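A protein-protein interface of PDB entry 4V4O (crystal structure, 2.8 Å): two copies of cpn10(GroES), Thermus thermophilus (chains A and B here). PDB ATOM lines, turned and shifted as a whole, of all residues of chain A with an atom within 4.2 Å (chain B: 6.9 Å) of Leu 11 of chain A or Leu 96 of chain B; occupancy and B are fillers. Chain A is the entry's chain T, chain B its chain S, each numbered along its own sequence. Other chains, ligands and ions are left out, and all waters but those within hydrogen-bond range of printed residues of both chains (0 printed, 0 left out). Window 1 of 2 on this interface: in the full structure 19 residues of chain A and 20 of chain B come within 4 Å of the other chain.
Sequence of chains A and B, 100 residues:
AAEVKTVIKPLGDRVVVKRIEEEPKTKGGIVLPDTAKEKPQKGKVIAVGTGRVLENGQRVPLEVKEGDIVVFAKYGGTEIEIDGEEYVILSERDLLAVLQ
Of the printed residues of chain A, Leu 96 of chain B touches Pro 10, Leu 11, Arg 14, Thr 78, Ile 80 and Ile 89.
Of the printed residues of chain B, Ile 80 of chain A touches Gln 41 (3.0 Å), Val 71 (3.8 Å) and Leu 96 (3.8 Å).
Printed residues of chain B within 4 Å of Pro 10 of chain A: Leu 96 (3.8 Å) and Ala 97 (3.5 Å).
Printed residues of chain B within 4 Å of Lys 9 of chain A: Ala 97 (3.1 Å) and Val 98 (2.5 Å).
Of the printed residues of chain B, Ile 89 of chain A touches Val 71 and Leu 96.
Of the printed residues of chain B, Thr 78 of chain A touches Ala 73 (3.8 Å) and Leu 96 (3.4 Å).
N of Gly 12 of chain A lies within hydrogen-bond range of OE1 of Glu 63 of chain B.
The side-chain carboxylate of Glu 63 of chain B is in hydrogen-bond range of the side-chain hydroxyl of Thr 50 of chain A (3.2 Å).
The guanidinium group (NH2) of Arg 14 of chain A lies within hydrogen-bond range of the backbone carbonyl oxygen (O) of Arg 93 of chain B (2.7 Å).
O of Leu 95 of chain B is in hydrogen-bond range of NE of Arg 14 of chain A (3.0 Å).
O of Val 98 of chain B is in hydrogen-bond range of N of Lys 9 of chain A, 2.5 Å away.
N of Phe 72 of chain B sits at hydrogen-bond distance from O of Gln 41 of chain B (2.9 Å).
The backbone carbonyl oxygen (O) of Val 71 of chain B is in hydrogen-bond range of the backbone NH (N) of Leu 96 of chain B (2.7 Å).
O of Ala 97 of chain B is in hydrogen-bond range of N of Val 71 of chain B, 3.2 Å away.
The backbone NH of Asp 13 of chain A is in hydrogen-bond range of the backbone carbonyl oxygen of Thr 50 of chain A (2.8 Å).
The backbone carbonyl oxygen of Thr 78 of chain A is in hydrogen-bond range of the backbone NH of Ile 89 of chain A (2.8 Å).
No position is printed for both chains.
Of the 21 pairs that touch across the chains among the printed residues, none has its exchanged pair printed and touching as well.
Among the printed residues, pairs that only touch across the chains: Lys 9 of chain A with Ala 97 of chain B (3.1 Å), Pro 10 of chain A with Leu 96 of chain B (3.8 Å), Pro 10 of chain A with Ala 97 of chain B (3.5 Å), Leu 11 of chain A with Glu 63 of chain B (3.5 Å), Leu 11 of chain A with Val 64 of chain B (3.9 Å), Leu 11 of chain A with Leu 95 of chain B (3.9 Å), Leu 11 of chain A with Leu 96 of chain B (3.5 Å), Arg 14 of chain A with Glu 92 of chain B (3.9 Å), Arg 14 of chain A with Leu 96 of chain B (3.1 Å), Thr 78 of chain A with Ala 73 of chain B (3.8 Å), Thr 78 of chain A with Leu 96 of chain B (3.4 Å), Ile 80 of chain A with Gln 41 of chain B (3.0 Å), Ile 80 of chain A with Val 71 of chain B (3.8 Å), Ile 80 of chain A with Leu 96 of chain B (3.8 Å), Ile 89 of chain A with Val 71 of chain B (3.8 Å) and Ile 89 of chain A with Leu 96 of chain B (3.2 Å).
Of the 10 printed residues of chain A, 9 touch a printed residue of chain B.
Hydrophobic or aromatic side chains of chain A within 4 Å of the printed part of chain B: Leu 11, Ile 80 and Ile 89.
Printed residues of chain B that touch a printed residue of chain A: Gln 41, Glu 63, Val 64, Val 71, Ala 73, Glu 92, Arg 93, Leu 95, Leu 96, Ala 97 and Val 98.
Hydrophobic or aromatic side chains of chain B that line the printed part of chain A: Val 64, Val 71, Ala 73, Leu 95, Leu 96, Ala 97 and Val 98.
Along chain B the printed residues that touch a printed residue of chain A span positions 41 to 98.
Among the printed residues, 21 pairs touch across the chains.
Among the printed residues, no Asp or Glu carboxylate lies within 4 Å of a Lys or Arg side-chain nitrogen of the other chain.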
ATOM      1  N   LYS A   9      -3.298   1.255  34.777  1.00  0.00           N
ATOM      2  CA  LYS A   9      -2.327   1.418  33.702  1.00  0.00           C
ATOM      3  C   LYS A   9      -2.721   0.664  32.444  1.00  0.00           C
ATOM      4  O   LYS A   9      -2.283  -0.475  32.218  1.00  0.00           O
ATOM      5  CB  LYS A   9      -0.941   0.951  34.149  1.00  0.00           C
ATOM      6  CG  LYS A   9      -0.247   1.878  35.139  1.00  0.00           C
ATOM      7  CD  LYS A   9       1.252   1.610  35.163  1.00  0.00           C
ATOM      8  CE  LYS A   9       1.975   2.498  36.152  1.00  0.00           C
ATOM      9  NZ  LYS A   9       1.722   3.939  35.982  1.00  0.00           N
ATOM     10  N   PRO A  10      -3.549   1.292  31.596  1.00  0.00           N
ATOM     11  CA  PRO A  10      -4.005   0.672  30.346  1.00  0.00           C
ATOM     12  C   PRO A  10      -2.852   0.347  29.422  1.00  0.00           C
ATOM     13  O   PRO A  10      -1.796   0.961  29.522  1.00  0.00           O
ATOM     14  CB  PRO A  10      -4.942   1.720  29.757  1.00  0.00           C
ATOM     15  CG  PRO A  10      -4.424   3.005  30.321  1.00  0.00           C
ATOM     16  CD  PRO A  10      -4.118   2.643  31.748  1.00  0.00           C
ATOM     17  N   LEU A  11      -3.056  -0.604  28.515  1.00  0.00           N
ATOM     18  CA  LEU A  11      -1.998  -0.989  27.592  1.00  0.00           C
ATOM     19  C   LEU A  11      -2.221  -0.536  26.145  1.00  0.00           C
ATOM     20  O   LEU A  11      -2.901   0.456  25.896  1.00  0.00           O
ATOM     21  CB  LEU A  11      -1.791  -2.502  27.651  1.00  0.00           C
ATOM     22  CG  LEU A  11      -1.362  -3.014  29.031  1.00  0.00           C
ATOM     23  CD1 LEU A  11      -1.154  -4.505  28.966  1.00  0.00           C
ATOM     24  CD2 LEU A  11      -0.078  -2.362  29.466  1.00  0.00           C
ATOM     25  N   GLY A  12      -1.643  -1.281  25.206  1.00  0.00           N
ATOM     26  CA  GLY A  12      -1.746  -0.959  23.791  1.00  0.00           C
ATOM     27  C   GLY A  12      -2.908  -0.115  23.299  1.00  0.00           C
ATOM     28  O   GLY A  12      -3.848  -0.638  22.745  1.00  0.00           O
ATOM     29  N   ASP A  13      -2.826   1.197  23.492  1.00  0.00           N
ATOM     30  CA  ASP A  13      -3.849   2.156  23.062  1.00  0.00           C
ATOM     31  C   ASP A  13      -5.189   2.031  23.786  1.00  0.00           C
ATOM     32  O   ASP A  13      -6.199   2.612  23.374  1.00  0.00           O
ATOM     33  CB  ASP A  13      -4.026   2.093  21.527  1.00  0.00           C
ATOM     34  CG  ASP A  13      -5.179   1.198  21.069  1.00  0.00           C
ATOM     35  OD1 ASP A  13      -5.840   0.552  21.906  1.00  0.00           O
ATOM     36  OD2 ASP A  13      -5.432   1.141  19.850  1.00  0.00           O
ATOM     37  N   ARG A  14      -5.207   1.250  24.855  1.00  0.00           N
ATOM     38  CA  ARG A  14      -6.411   1.085  25.643  1.00  0.00           C
ATOM     39  C   ARG A  14      -6.575   2.294  26.556  1.00  0.00           C
ATOM     40  O   ARG A  14      -5.615   2.749  27.168  1.00  0.00           O
ATOM     41  CB  ARG A  14      -6.316  -0.171  26.504  1.00  0.00           C
ATOM     42  CG  ARG A  14      -6.352  -1.483  25.742  1.00  0.00           C
ATOM     43  CD  ARG A  14      -5.570  -2.522  26.534  1.00  0.00           C
ATOM     44  NE  ARG A  14      -5.800  -3.918  26.155  1.00  0.00           N
ATOM     45  CZ  ARG A  14      -5.690  -4.403  24.925  1.00  0.00           C
ATOM     46  NH1 ARG A  14      -5.358  -3.602  23.930  1.00  0.00           N
ATOM     47  NH2 ARG A  14      -5.894  -5.694  24.696  1.00  0.00           N
ATOM     48  N   THR A  50      -0.042   3.512  26.644  1.00  0.00           N
ATOM     49  CA  THR A  50       0.987   3.530  25.607  1.00  0.00           C
ATOM     50  C   THR A  50       0.228   3.578  24.290  1.00  0.00           C
ATOM     51  O   THR A  50      -0.831   3.005  24.195  1.00  0.00           O
ATOM     52  CB  THR A  50       1.779   2.208  25.645  1.00  0.00           C
ATOM     53  OG1 THR A  50       2.535   2.136  26.855  1.00  0.00           O
ATOM     54  CG2 THR A  50       2.691   2.081  24.452  1.00  0.00           C
ATOM     55  N   THR A  78     -14.289  -4.410  27.493  1.00  0.00           N
ATOM     56  CA  THR A  78     -14.414  -5.003  28.828  1.00  0.00           C
ATOM     57  C   THR A  78     -14.700  -3.945  29.905  1.00  0.00           C
ATOM     58  O   THR A  78     -14.376  -2.766  29.735  1.00  0.00           O
ATOM     59  CB  THR A  78     -13.121  -5.774  29.210  1.00  0.00           C
ATOM     60  OG1 THR A  78     -12.881  -6.816  28.250  1.00  0.00           O
ATOM     61  CG2 THR A  78     -13.248  -6.386  30.600  1.00  0.00           C
ATOM     62  N   ILE A  80     -14.697  -3.226  34.337  1.00  0.00           N
ATOM     63  CA  ILE A  80     -14.201  -3.686  35.632  1.00  0.00           C
ATOM     64  C   ILE A  80     -14.348  -2.614  36.709  1.00  0.00           C
ATOM     65  O   ILE A  80     -14.456  -1.422  36.415  1.00  0.00           O
ATOM     66  CB  ILE A  80     -12.706  -4.110  35.580  1.00  0.00           C
ATOM     67  CG1 ILE A  80     -12.507  -5.262  34.593  1.00  0.00           C
ATOM     68  CG2 ILE A  80     -12.236  -4.558  36.962  1.00  0.00           C
ATOM     69  CD1 ILE A  80     -12.073  -4.823  33.219  1.00  0.00           C
ATOM     70  N   ILE A  89     -12.613  -0.546  29.926  1.00  0.00           N
ATOM     71  CA  ILE A  89     -11.348  -0.593  29.213  1.00  0.00           C
ATOM     72  C   ILE A  89     -11.639  -0.765  27.724  1.00  0.00           C
ATOM     73  O   ILE A  89     -11.822  -1.881  27.234  1.00  0.00           O
ATOM     74  CB  ILE A  89     -10.471  -1.773  29.716  1.00  0.00           C
ATOM     75  CG1 ILE A  89      -9.972  -1.479  31.136  1.00  0.00           C
ATOM     76  CG2 ILE A  89      -9.297  -2.007  28.770  1.00  0.00           C
ATOM     77  CD1 ILE A  89      -9.213  -2.637  31.783  1.00  0.00           C
ATOM     78  N   GLN B  41     -10.422 -11.082  37.986  1.00  0.00           N
ATOM     79  CA  GLN B  41      -9.917 -10.611  36.714  1.00  0.00           C
ATOM     80  C   GLN B  41      -8.522 -10.063  36.968  1.00  0.00           C
ATOM     81  O   GLN B  41      -7.933  -9.433  36.098  1.00  0.00           O
ATOM     82  CB  GLN B  41     -10.815  -9.499  36.173  1.00  0.00           C
ATOM     83  CG  GLN B  41     -12.249  -9.914  35.904  1.00  0.00           C
ATOM     84  CD  GLN B  41     -13.094  -8.761  35.388  1.00  0.00           C
ATOM     85  OE1 GLN B  41     -13.263  -7.752  36.069  1.00  0.00           O
ATOM     86  NE2 GLN B  41     -13.624  -8.905  34.178  1.00  0.00           N
ATOM     87  N   LEU B  62       6.584  -7.311  25.720  1.00  0.00           N
ATOM     88  CA  LEU B  62       5.328  -7.231  26.441  1.00  0.00           C
ATOM     89  C   LEU B  62       5.358  -6.001  27.342  1.00  0.00           C
ATOM     90  O   LEU B  62       6.292  -5.838  28.126  1.00  0.00           O
ATOM     91  CB  LEU B  62       5.152  -8.496  27.277  1.00  0.00           C
ATOM     92  CG  LEU B  62       5.295  -9.763  26.433  1.00  0.00           C
ATOM     93  CD1 LEU B  62       5.494 -10.945  27.332  1.00  0.00           C
ATOM     94  CD2 LEU B  62       4.074  -9.941  25.551  1.00  0.00           C
ATOM     95  N   GLU B  63       4.348  -5.136  27.228  1.00  0.00           N
ATOM     96  CA  GLU B  63       4.275  -3.922  28.044  1.00  0.00           C
ATOM     97  C   GLU B  63       4.171  -4.250  29.534  1.00  0.00           C
ATOM     98  O   GLU B  63       4.059  -3.344  30.378  1.00  0.00           O
ATOM     99  CB  GLU B  63       3.064  -3.069  27.638  1.00  0.00           C
ATOM    100  CG  GLU B  63       2.909  -2.856  26.142  1.00  0.00           C
ATOM    101  CD  GLU B  63       1.934  -1.741  25.816  1.00  0.00           C
ATOM    102  OE1 GLU B  63       1.481  -1.653  24.663  1.00  0.00           O
ATOM    103  OE2 GLU B  63       1.620  -0.934  26.706  1.00  0.00           O
ATOM    104  N   VAL B  64       4.223  -5.541  29.860  1.00  0.00           N
ATOM    105  CA  VAL B  64       4.097  -5.980  31.245  1.00  0.00           C
ATOM    106  C   VAL B  64       5.323  -6.628  31.849  1.00  0.00           C
ATOM    107  O   VAL B  64       5.870  -7.607  31.331  1.00  0.00           O
ATOM    108  CB  VAL B  64       2.915  -6.946  31.409  1.00  0.00           C
ATOM    109  CG1 VAL B  64       2.853  -7.439  32.844  1.00  0.00           C
ATOM    110  CG2 VAL B  64       1.617  -6.240  31.035  1.00  0.00           C
ATOM    111  N   VAL B  70      -2.076  -7.392  37.024  1.00  0.00           N
ATOM    112  CA  VAL B  70      -2.777  -7.280  35.746  1.00  0.00           C
ATOM    113  C   VAL B  70      -4.290  -7.482  35.783  1.00  0.00           C
ATOM    114  O   VAL B  70      -4.810  -8.268  36.574  1.00  0.00           O
ATOM    115  CB  VAL B  70      -2.213  -8.281  34.728  1.00  0.00           C
ATOM    116  CG1 VAL B  70      -2.657  -7.898  33.326  1.00  0.00           C
ATOM    117  CG2 VAL B  70      -0.704  -8.328  34.833  1.00  0.00           C
ATOM    118  N   VAL B  71      -4.972  -6.765  34.891  1.00  0.00           N
ATOM    119  CA  VAL B  71      -6.423  -6.804  34.732  1.00  0.00           C
ATOM    120  C   VAL B  71      -6.745  -7.396  33.364  1.00  0.00           C
ATOM    121  O   VAL B  71      -6.386  -6.829  32.336  1.00  0.00           O
ATOM    122  CB  VAL B  71      -7.028  -5.382  34.804  1.00  0.00           C
ATOM    123  CG1 VAL B  71      -8.448  -5.380  34.247  1.00  0.00           C
ATOM    124  CG2 VAL B  71      -7.026  -4.893  36.238  1.00  0.00           C
ATOM    125  N   PHE B  72      -7.436  -8.526  33.350  1.00  0.00           N
ATOM    126  CA  PHE B  72      -7.778  -9.183  32.098  1.00  0.00           C
ATOM    127  C   PHE B  72      -9.225  -9.663  32.091  1.00  0.00           C
ATOM    128  O   PHE B  72      -9.836  -9.836  33.145  1.00  0.00           O
ATOM    129  CB  PHE B  72      -6.844 -10.366  31.895  1.00  0.00           C
ATOM    130  CG  PHE B  72      -6.924 -11.385  32.991  1.00  0.00           C
ATOM    131  CD1 PHE B  72      -7.661 -12.551  32.822  1.00  0.00           C
ATOM    132  CD2 PHE B  72      -6.281 -11.170  34.203  1.00  0.00           C
ATOM    133  CE1 PHE B  72      -7.755 -13.488  33.845  1.00  0.00           C
ATOM    134  CE2 PHE B  72      -6.370 -12.100  35.231  1.00  0.00           C
ATOM    135  CZ  PHE B  72      -7.109 -13.262  35.052  1.00  0.00           C
ATOM    136  N   ALA B  73      -9.771  -9.872  30.897  1.00  0.00           N
ATOM    137  CA  ALA B  73     -11.137 -10.355  30.767  1.00  0.00           C
ATOM    138  C   ALA B  73     -11.171 -11.812  31.242  1.00  0.00           C
ATOM    139  O   ALA B  73     -11.060 -12.744  30.442  1.00  0.00           O
ATOM    140  CB  ALA B  73     -11.587 -10.251  29.319  1.00  0.00           C
ATOM    141  N   LYS B  74     -11.314 -11.975  32.558  1.00  0.00           N
ATOM    142  CA  LYS B  74     -11.360 -13.265  33.262  1.00  0.00           C
ATOM    143  C   LYS B  74     -11.809 -14.496  32.478  1.00  0.00           C
ATOM    144  O   LYS B  74     -11.425 -15.620  32.810  1.00  0.00           O
ATOM    145  CB  LYS B  74     -12.262 -13.135  34.491  1.00  0.00           C
ATOM    146  CG  LYS B  74     -13.678 -12.721  34.114  1.00  0.00           C
ATOM    147  CD  LYS B  74     -14.615 -12.625  35.300  1.00  0.00           C
ATOM    148  CE  LYS B  74     -15.987 -12.169  34.830  1.00  0.00           C
ATOM    149  NZ  LYS B  74     -16.943 -12.028  35.953  1.00  0.00           N
ATOM    150  N   SER B  91      -2.775 -14.056  26.782  1.00  0.00           N
ATOM    151  CA  SER B  91      -2.041 -13.413  25.711  1.00  0.00           C
ATOM    152  C   SER B  91      -2.117 -11.931  26.009  1.00  0.00           C
ATOM    153  O   SER B  91      -2.748 -11.512  26.974  1.00  0.00           O
ATOM    154  CB  SER B  91      -2.660 -13.706  24.344  1.00  0.00           C
ATOM    155  OG  SER B  91      -2.310 -15.006  23.900  1.00  0.00           O
ATOM    156  N   GLU B  92      -1.466 -11.141  25.177  1.00  0.00           N
ATOM    157  CA  GLU B  92      -1.435  -9.705  25.356  1.00  0.00           C
ATOM    158  C   GLU B  92      -2.826  -9.126  25.159  1.00  0.00           C
ATOM    159  O   GLU B  92      -3.236  -8.217  25.883  1.00  0.00           O
ATOM    160  CB  GLU B  92      -0.457  -9.130  24.345  1.00  0.00           C
ATOM    161  CG  GLU B  92      -0.165  -7.666  24.436  1.00  0.00           C
ATOM    162  CD  GLU B  92       0.899  -7.264  23.436  1.00  0.00           C
ATOM    163  OE1 GLU B  92       1.269  -8.100  22.592  1.00  0.00           O
ATOM    164  OE2 GLU B  92       1.368  -6.114  23.480  1.00  0.00           O
ATOM    165  N   ARG B  93      -3.552  -9.667  24.183  1.00  0.00           N
ATOM    166  CA  ARG B  93      -4.899  -9.198  23.893  1.00  0.00           C
ATOM    167  C   ARG B  93      -5.711  -9.197  25.174  1.00  0.00           C
ATOM    168  O   ARG B  93      -6.323  -8.197  25.538  1.00  0.00           O
ATOM    169  CB  ARG B  93      -5.581 -10.114  22.878  1.00  0.00           C
ATOM    170  CG  ARG B  93      -4.841 -10.290  21.570  1.00  0.00           C
ATOM    171  CD  ARG B  93      -5.740 -10.971  20.546  1.00  0.00           C
ATOM    172  NE  ARG B  93      -5.105 -11.089  19.236  1.00  0.00           N
ATOM    173  CZ  ARG B  93      -4.213 -12.019  18.916  1.00  0.00           C
ATOM    174  NH1 ARG B  93      -3.852 -12.923  19.812  1.00  0.00           N
ATOM    175  NH2 ARG B  93      -3.677 -12.042  17.704  1.00  0.00           N
ATOM    176  N   ASP B  94      -5.695 -10.333  25.859  1.00  0.00           N
ATOM    177  CA  ASP B  94      -6.438 -10.501  27.097  1.00  0.00           C
ATOM    178  C   ASP B  94      -6.029  -9.505  28.183  1.00  0.00           C
ATOM    179  O   ASP B  94      -6.841  -9.149  29.039  1.00  0.00           O
ATOM    180  CB  ASP B  94      -6.276 -11.940  27.602  1.00  0.00           C
ATOM    181  CG  ASP B  94      -6.551 -12.979  26.516  1.00  0.00           C
ATOM    182  OD1 ASP B  94      -7.430 -12.732  25.655  1.00  0.00           O
ATOM    183  OD2 ASP B  94      -5.898 -14.046  26.530  1.00  0.00           O
ATOM    184  N   LEU B  95      -4.776  -9.054  28.146  1.00  0.00           N
ATOM    185  CA  LEU B  95      -4.280  -8.090  29.128  1.00  0.00           C
ATOM    186  C   LEU B  95      -4.887  -6.724  28.823  1.00  0.00           C
ATOM    187  O   LEU B  95      -4.656  -6.143  27.764  1.00  0.00           O
ATOM    188  CB  LEU B  95      -2.764  -8.030  29.065  1.00  0.00           C
ATOM    189  CG  LEU B  95      -2.146  -9.409  29.280  1.00  0.00           C
ATOM    190  CD1 LEU B  95      -0.655  -9.357  29.046  1.00  0.00           C
ATOM    191  CD2 LEU B  95      -2.450  -9.882  30.684  1.00  0.00           C
ATOM    192  N   LEU B  96      -5.667  -6.217  29.765  1.00  0.00           N
ATOM    193  CA  LEU B  96      -6.358  -4.955  29.586  1.00  0.00           C
ATOM    194  C   LEU B  96      -5.636  -3.750  30.173  1.00  0.00           C
ATOM    195  O   LEU B  96      -5.712  -2.652  29.623  1.00  0.00           O
ATOM    196  CB  LEU B  96      -7.764  -5.064  30.190  1.00  0.00           C
ATOM    197  CG  LEU B  96      -8.662  -6.169  29.619  1.00  0.00           C
ATOM    198  CD1 LEU B  96      -9.899  -6.348  30.491  1.00  0.00           C
ATOM    199  CD2 LEU B  96      -9.049  -5.814  28.196  1.00  0.00           C
ATOM    200  N   ALA B  97      -4.940  -3.946  31.286  1.00  0.00           N
ATOM    201  CA  ALA B  97      -4.234  -2.844  31.938  1.00  0.00           C
ATOM    202  C   ALA B  97      -3.414  -3.363  33.103  1.00  0.00           C
ATOM    203  O   ALA B  97      -3.303  -4.573  33.304  1.00  0.00           O
ATOM    204  CB  ALA B  97      -5.237  -1.805  32.439  1.00  0.00           C
ATOM    205  N   VAL B  98      -2.837  -2.446  33.873  1.00  0.00           N
ATOM    206  CA  VAL B  98      -2.041  -2.838  35.022  1.00  0.00           C
ATOM    207  C   VAL B  98      -2.373  -1.942  36.206  1.00  0.00           C
ATOM    208  O   VAL B  98      -2.645  -0.755  36.034  1.00  0.00           O
ATOM    209  CB  VAL B  98      -0.542  -2.750  34.708  1.00  0.00           C
ATOM    210  CG1 VAL B  98       0.256  -3.284  35.877  1.00  0.00           C
ATOM    211  CG2 VAL B  98      -0.227  -3.551  33.453  1.00  0.00           C
